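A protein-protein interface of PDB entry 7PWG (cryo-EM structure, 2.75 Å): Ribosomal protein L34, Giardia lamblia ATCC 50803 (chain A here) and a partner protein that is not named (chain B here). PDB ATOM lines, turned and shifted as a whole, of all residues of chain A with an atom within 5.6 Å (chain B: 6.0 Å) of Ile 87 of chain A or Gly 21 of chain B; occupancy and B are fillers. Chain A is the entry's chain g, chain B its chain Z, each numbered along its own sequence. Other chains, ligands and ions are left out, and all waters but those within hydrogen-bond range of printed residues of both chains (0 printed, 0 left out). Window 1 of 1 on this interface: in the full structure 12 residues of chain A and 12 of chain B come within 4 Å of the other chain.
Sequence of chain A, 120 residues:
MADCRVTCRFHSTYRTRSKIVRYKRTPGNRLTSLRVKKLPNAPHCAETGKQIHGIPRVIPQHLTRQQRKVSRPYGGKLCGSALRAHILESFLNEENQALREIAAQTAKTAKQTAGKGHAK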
ATOM      1  N   ALA A  82     -23.036  16.742  16.253  1.00  0.00           N
ATOM      2  CA  ALA A  82     -21.709  16.753  16.844  1.00  0.00           C
ATOM      3  C   ALA A  82     -21.228  15.347  17.162  1.00  0.00           C
ATOM      4  O   ALA A  82     -20.025  15.087  17.128  1.00  0.00           O
ATOM      5  CB  ALA A  82     -21.702  17.617  18.099  1.00  0.00           C
ATOM      6  N   LEU A  83     -22.140  14.432  17.487  1.00  0.00           N
ATOM      7  CA  LEU A  83     -21.741  13.049  17.705  1.00  0.00           C
ATOM      8  C   LEU A  83     -21.223  12.430  16.418  1.00  0.00           C
ATOM      9  O   LEU A  83     -20.139  11.839  16.396  1.00  0.00           O
ATOM     10  CB  LEU A  83     -22.910  12.241  18.255  1.00  0.00           C
ATOM     11  CG  LEU A  83     -22.668  10.739  18.387  1.00  0.00           C
ATOM     12  CD1 LEU A  83     -21.463  10.470  19.273  1.00  0.00           C
ATOM     13  CD2 LEU A  83     -23.898  10.034  18.929  1.00  0.00           C
ATOM     14  N   ARG A  84     -21.973  12.583  15.331  1.00  0.00           N
ATOM     15  CA  ARG A  84     -21.590  11.985  14.060  1.00  0.00           C
ATOM     16  C   ARG A  84     -20.243  12.501  13.567  1.00  0.00           C
ATOM     17  O   ARG A  84     -19.510  11.774  12.888  1.00  0.00           O
ATOM     18  CB  ARG A  84     -22.681  12.256  13.034  1.00  0.00           C
ATOM     19  CG  ARG A  84     -22.419  11.694  11.669  1.00  0.00           C
ATOM     20  CD  ARG A  84     -23.493  12.145  10.716  1.00  0.00           C
ATOM     21  NE  ARG A  84     -23.304  11.603   9.386  1.00  0.00           N
ATOM     22  CZ  ARG A  84     -22.592  12.198   8.442  1.00  0.00           C
ATOM     23  NH1 ARG A  84     -22.014  13.360   8.685  1.00  0.00           N
ATOM     24  NH2 ARG A  84     -22.457  11.631   7.253  1.00  0.00           N
ATOM     25  N   ALA A  85     -19.901  13.743  13.884  1.00  0.00           N
ATOM     26  CA  ALA A  85     -18.617  14.283  13.471  1.00  0.00           C
ATOM     27  C   ALA A  85     -17.475  13.763  14.334  1.00  0.00           C
ATOM     28  O   ALA A  85     -16.362  13.595  13.834  1.00  0.00           O
ATOM     29  CB  ALA A  85     -18.661  15.808  13.500  1.00  0.00           C
ATOM     30  N   HIS A  86     -17.722  13.528  15.624  1.00  0.00           N
ATOM     31  CA  HIS A  86     -16.721  12.892  16.471  1.00  0.00           C
ATOM     32  C   HIS A  86     -16.470  11.451  16.048  1.00  0.00           C
ATOM     33  O   HIS A  86     -15.333  10.977  16.096  1.00  0.00           O
ATOM     34  CB  HIS A  86     -17.149  12.931  17.934  1.00  0.00           C
ATOM     35  CG  HIS A  86     -16.814  14.204  18.637  1.00  0.00           C
ATOM     36  ND1 HIS A  86     -15.545  14.491  19.087  1.00  0.00           N
ATOM     37  CD2 HIS A  86     -17.587  15.252  19.000  1.00  0.00           C
ATOM     38  CE1 HIS A  86     -15.548  15.670  19.679  1.00  0.00           C
ATOM     39  NE2 HIS A  86     -16.776  16.152  19.641  1.00  0.00           N
ATOM     40  N   ILE A  87     -17.523  10.738  15.654  1.00  0.00           N
ATOM     41  CA  ILE A  87     -17.386   9.343  15.254  1.00  0.00           C
ATOM     42  C   ILE A  87     -16.530   9.229  14.004  1.00  0.00           C
ATOM     43  O   ILE A  87     -15.676   8.342  13.899  1.00  0.00           O
ATOM     44  CB  ILE A  87     -18.775   8.712  15.049  1.00  0.00           C
ATOM     45  CG1 ILE A  87     -19.569   8.736  16.352  1.00  0.00           C
ATOM     46  CG2 ILE A  87     -18.659   7.311  14.509  1.00  0.00           C
ATOM     47  CD1 ILE A  87     -21.016   8.357  16.179  1.00  0.00           C
ATOM     48  N   LEU A  88     -16.745  10.118  13.035  1.00  0.00           N
ATOM     49  CA  LEU A  88     -15.972  10.073  11.799  1.00  0.00           C
ATOM     50  C   LEU A  88     -14.521  10.461  12.033  1.00  0.00           C
ATOM     51  O   LEU A  88     -13.613   9.849  11.464  1.00  0.00           O
ATOM     52  CB  LEU A  88     -16.597  10.990  10.753  1.00  0.00           C
ATOM     53  CG  LEU A  88     -17.557  10.349   9.764  1.00  0.00           C
ATOM     54  CD1 LEU A  88     -18.566   9.526  10.499  1.00  0.00           C
ATOM     55  CD2 LEU A  88     -18.258  11.402   8.943  1.00  0.00           C
ATOM     56  N   GLU A  89     -14.278  11.486  12.844  1.00  0.00           N
ATOM     57  CA  GLU A  89     -12.904  11.875  13.121  1.00  0.00           C
ATOM     58  C   GLU A  89     -12.144  10.743  13.791  1.00  0.00           C
ATOM     59  O   GLU A  89     -11.024  10.413  13.393  1.00  0.00           O
ATOM     60  CB  GLU A  89     -12.871  13.130  13.981  1.00  0.00           C
ATOM     61  CG  GLU A  89     -13.013  14.397  13.196  1.00  0.00           C
ATOM     62  CD  GLU A  89     -11.827  15.318  13.357  1.00  0.00           C
ATOM     63  OE1 GLU A  89     -10.909  14.969  14.132  1.00  0.00           O
ATOM     64  OE2 GLU A  89     -11.819  16.384  12.709  1.00  0.00           O
ATOM     65  N   SER A  90     -12.753  10.110  14.793  1.00  0.00           N
ATOM     66  CA  SER A  90     -12.100   8.992  15.459  1.00  0.00           C
ATOM     67  C   SER A  90     -11.764   7.873  14.479  1.00  0.00           C
ATOM     68  O   SER A  90     -10.617   7.423  14.403  1.00  0.00           O
ATOM     69  CB  SER A  90     -12.983   8.470  16.584  1.00  0.00           C
ATOM     70  OG  SER A  90     -12.450   7.279  17.120  1.00  0.00           O
ATOM     71  N   PHE A  91     -12.746   7.422  13.706  1.00  0.00           N
ATOM     72  CA  PHE A  91     -12.514   6.286  12.824  1.00  0.00           C
ATOM     73  C   PHE A  91     -11.490   6.605  11.737  1.00  0.00           C
ATOM     74  O   PHE A  91     -10.638   5.767  11.427  1.00  0.00           O
ATOM     75  CB  PHE A  91     -13.828   5.811  12.207  1.00  0.00           C
ATOM     76  CG  PHE A  91     -13.641   4.899  11.041  1.00  0.00           C
ATOM     77  CD1 PHE A  91     -12.962   3.702  11.184  1.00  0.00           C
ATOM     78  CD2 PHE A  91     -14.129   5.239   9.789  1.00  0.00           C
ATOM     79  CE1 PHE A  91     -12.772   2.865  10.094  1.00  0.00           C
ATOM     80  CE2 PHE A  91     -13.953   4.403   8.706  1.00  0.00           C
ATOM     81  CZ  PHE A  91     -13.270   3.217   8.857  1.00  0.00           C
ATOM     82  N   LEU A  92     -11.547   7.802  11.148  1.00  0.00           N
ATOM     83  CA  LEU A  92     -10.684   8.120  10.010  1.00  0.00           C
ATOM     84  C   LEU A  92      -9.247   8.418  10.410  1.00  0.00           C
ATOM     85  O   LEU A  92      -8.332   8.159   9.627  1.00  0.00           O
ATOM     86  CB  LEU A  92     -11.238   9.309   9.232  1.00  0.00           C
ATOM     87  CG  LEU A  92     -12.480   9.070   8.389  1.00  0.00           C
ATOM     88  CD1 LEU A  92     -12.950  10.378   7.811  1.00  0.00           C
ATOM     89  CD2 LEU A  92     -12.196   8.080   7.292  1.00  0.00           C
ATOM     90  N   ILE B  13     -19.819   1.220  10.474  1.00  0.00           N
ATOM     91  CA  ILE B  13     -19.979   1.915  11.748  1.00  0.00           C
ATOM     92  C   ILE B  13     -21.339   2.602  11.732  1.00  0.00           C
ATOM     93  O   ILE B  13     -21.720   3.208  10.726  1.00  0.00           O
ATOM     94  CB  ILE B  13     -18.842   2.923  11.978  1.00  0.00           C
ATOM     95  CG1 ILE B  13     -17.484   2.277  11.706  1.00  0.00           C
ATOM     96  CG2 ILE B  13     -18.872   3.463  13.388  1.00  0.00           C
ATOM     97  CD1 ILE B  13     -16.760   1.784  12.931  1.00  0.00           C
ATOM     98  N   VAL B  14     -22.085   2.483  12.831  1.00  0.00           N
ATOM     99  CA  VAL B  14     -23.406   3.097  12.941  1.00  0.00           C
ATOM    100  C   VAL B  14     -23.251   4.558  13.340  1.00  0.00           C
ATOM    101  O   VAL B  14     -22.471   4.887  14.235  1.00  0.00           O
ATOM    102  CB  VAL B  14     -24.275   2.326  13.949  1.00  0.00           C
ATOM    103  CG1 VAL B  14     -25.605   2.968  14.097  1.00  0.00           C
ATOM    104  CG2 VAL B  14     -24.445   0.879  13.516  1.00  0.00           C
ATOM    105  N   LEU B  15     -24.000   5.445  12.678  1.00  0.00           N
ATOM    106  CA  LEU B  15     -23.833   6.886  12.841  1.00  0.00           C
ATOM    107  C   LEU B  15     -24.964   7.590  13.580  1.00  0.00           C
ATOM    108  O   LEU B  15     -24.709   8.618  14.205  1.00  0.00           O
ATOM    109  CB  LEU B  15     -23.660   7.557  11.474  1.00  0.00           C
ATOM    110  CG  LEU B  15     -22.333   7.280  10.772  1.00  0.00           C
ATOM    111  CD1 LEU B  15     -22.220   8.049   9.479  1.00  0.00           C
ATOM    112  CD2 LEU B  15     -21.200   7.612  11.700  1.00  0.00           C
ATOM    113  N   GLN B  16     -26.201   7.100  13.516  1.00  0.00           N
ATOM    114  CA  GLN B  16     -27.322   7.742  14.196  1.00  0.00           C
ATOM    115  C   GLN B  16     -28.163   6.697  14.922  1.00  0.00           C
ATOM    116  O   GLN B  16     -28.139   5.515  14.585  1.00  0.00           O
ATOM    117  CB  GLN B  16     -28.199   8.530  13.212  1.00  0.00           C
ATOM    118  CG  GLN B  16     -27.409   9.349  12.197  1.00  0.00           C
ATOM    119  CD  GLN B  16     -28.241  10.361  11.462  1.00  0.00           C
ATOM    120  OE1 GLN B  16     -29.425  10.519  11.724  1.00  0.00           O
ATOM    121  NE2 GLN B  16     -27.616  11.070  10.542  1.00  0.00           N
ATOM    122  N   HIS B  19     -27.694   3.167  18.689  1.00  0.00           N
ATOM    123  CA  HIS B  19     -26.467   2.393  18.571  1.00  0.00           C
ATOM    124  C   HIS B  19     -25.374   3.145  17.823  1.00  0.00           C
ATOM    125  O   HIS B  19     -24.542   2.530  17.159  1.00  0.00           O
ATOM    126  CB  HIS B  19     -26.745   1.053  17.893  1.00  0.00           C
ATOM    127  CG  HIS B  19     -27.896   0.304  18.487  1.00  0.00           C
ATOM    128  ND1 HIS B  19     -27.878  -0.192  19.770  1.00  0.00           N
ATOM    129  CD2 HIS B  19     -29.105  -0.028  17.974  1.00  0.00           C
ATOM    130  CE1 HIS B  19     -29.025  -0.794  20.026  1.00  0.00           C
ATOM    131  NE2 HIS B  19     -29.789  -0.704  18.953  1.00  0.00           N
ATOM    132  N   ALA B  20     -25.363   4.468  17.912  1.00  0.00           N
ATOM    133  CA  ALA B  20     -24.367   5.251  17.198  1.00  0.00           C
ATOM    134  C   ALA B  20     -22.971   4.970  17.737  1.00  0.00           C
ATOM    135  O   ALA B  20     -22.762   4.869  18.945  1.00  0.00           O
ATOM    136  CB  ALA B  20     -24.678   6.738  17.308  1.00  0.00           C
ATOM    137  N   GLY B  21     -22.011   4.858  16.831  1.00  0.00           N
ATOM    138  CA  GLY B  21     -20.652   4.543  17.209  1.00  0.00           C
ATOM    139  C   GLY B  21     -20.376   3.089  17.508  1.00  0.00           C
ATOM    140  O   GLY B  21     -19.330   2.792  18.086  1.00  0.00           O
ATOM    141  N   LYS B  22     -21.276   2.177  17.148  1.00  0.00           N
ATOM    142  CA  LYS B  22     -21.084   0.747  17.344  1.00  0.00           C
ATOM    143  C   LYS B  22     -21.009   0.040  16.000  1.00  0.00           C
ATOM    144  O   LYS B  22     -21.576   0.499  15.009  1.00  0.00           O
ATOM    145  CB  LYS B  22     -22.214   0.139  18.178  1.00  0.00           C
ATOM    146  CG  LYS B  22     -22.382   0.747  19.554  1.00  0.00           C
ATOM    147  CD  LYS B  22     -23.759   0.427  20.097  1.00  0.00           C
ATOM    148  CE  LYS B  22     -23.906   0.794  21.546  1.00  0.00           C
ATOM    149  NZ  LYS B  22     -25.210   0.304  22.067  1.00  0.00           N
ATOM    150  N   LYS B  23     -20.317  -1.092  15.975  1.00  0.00           N
ATOM    151  CA  LYS B  23     -20.039  -1.805  14.736  1.00  0.00           C
ATOM    152  C   LYS B  23     -21.140  -2.802  14.409  1.00  0.00           C
ATOM    153  O   LYS B  23     -21.861  -3.276  15.288  1.00  0.00           O
ATOM    154  CB  LYS B  23     -18.704  -2.533  14.825  1.00  0.00           C
ATOM    155  CG  LYS B  23     -17.567  -1.678  15.304  1.00  0.00           C
ATOM    156  CD  LYS B  23     -16.254  -2.258  14.852  1.00  0.00           C
ATOM    157  CE  LYS B  23     -15.117  -1.712  15.654  1.00  0.00           C
ATOM    158  NZ  LYS B  23     -15.161  -0.247  15.720  1.00  0.00           N
ATOM    159  N   LEU B 131     -14.494   1.375  19.581  1.00  0.00           N
ATOM    160  CA  LEU B 131     -13.870   2.513  18.900  1.00  0.00           C
ATOM    161  C   LEU B 131     -13.784   3.708  19.844  1.00  0.00           C
ATOM    162  O   LEU B 131     -14.804   4.122  20.393  1.00  0.00           O
ATOM    163  CB  LEU B 131     -14.657   2.869  17.641  1.00  0.00           C
ATOM    164  CG  LEU B 131     -14.470   4.227  16.959  1.00  0.00           C
ATOM    165  CD1 LEU B 131     -13.209   4.292  16.129  1.00  0.00           C
ATOM    166  CD2 LEU B 131     -15.663   4.572  16.099  1.00  0.00           C
ATOM    167  N   ILE B 133     -13.566   7.452  21.392  1.00  0.00           N
ATOM    168  CA  ILE B 133     -14.211   8.695  20.981  1.00  0.00           C
ATOM    169  C   ILE B 133     -13.883   9.807  21.972  1.00  0.00           C
ATOM    170  O   ILE B 133     -13.997   9.617  23.185  1.00  0.00           O
ATOM    171  CB  ILE B 133     -15.743   8.527  20.871  1.00  0.00           C
ATOM    172  CG1 ILE B 133     -16.104   7.349  19.971  1.00  0.00           C
ATOM    173  CG2 ILE B 133     -16.391   9.775  20.343  1.00  0.00           C
ATOM    174  CD1 ILE B 133     -17.538   6.932  20.071  1.00  0.00           C
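Of the 11 printed residues of chain B, 4 touch a printed residue of chain A.
Hydrophobic or aromatic side chains of chain B that line the printed part of chain A: Leu 15, Ala 20 and Leu 131.
Printed residues of chain A that touch a printed residue of chain B: Leu 83, Arg 84, Ile 87, Leu 88, Ser 90 and Phe 91.
Hydrophobic or aromatic side chains of chain A that line the printed part of chain B: Leu 83, Ile 87 and Leu 88.
Among the printed residues, 7 pairs touch across the chains.
Among the printed residues, no Asp or Glu carboxylate lies within 4 Å of a Lys or Arg side-chain nitrogen of the other chain.
O of Val 14 of chain B lies within hydrogen-bond range of N of Gly 21 of chain B, at 2.6 Å.
Of the printed residues of chain B, Ile 87 of chain A touches Leu 15 (3.8 Å) and Gly 21 (3.7 Å).
Gly 21 of chain B touches one residue of chain A.
Printed residues of chain B within 4 Å of Leu 83 of chain A: Ala 20.
Of the printed residues of chain B, Leu 88 of chain A touches Leu 15.
Printed residues of chain A within 4 Å of Ala 20 of chain B: Leu 83.
Of the printed residues of chain B, Phe 91 of chain A touches Leu 131 (3.9 Å).
Ile 13 of chain B touches none of the printed residues of chain A.
Gln 16 of chain B touches none of the printed residues of chain A.
The nearest printed residue of chain B that does not touch Leu 83 of chain A is Leu 15 of chain B (5.0 Å).
Among the printed residues, merely in contact across the chains: Leu 83 of chain A with Ala 20 of chain B (3.8 Å), Arg 84 of chain A with Leu 15 of chain B (3.7 Å), Ile 87 of chain A with Leu 15 of chain B (3.8 Å), Ile 87 of chain A with Gly 21 of chain B (3.7 Å), Leu 88 of chain A with Leu 15 of chain B (3.5 Å), Ser 90 of chain A with Leu 131 of chain B (3.2 Å) and Phe 91 of chain A with Leu 131 of chain B (3.9 Å).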
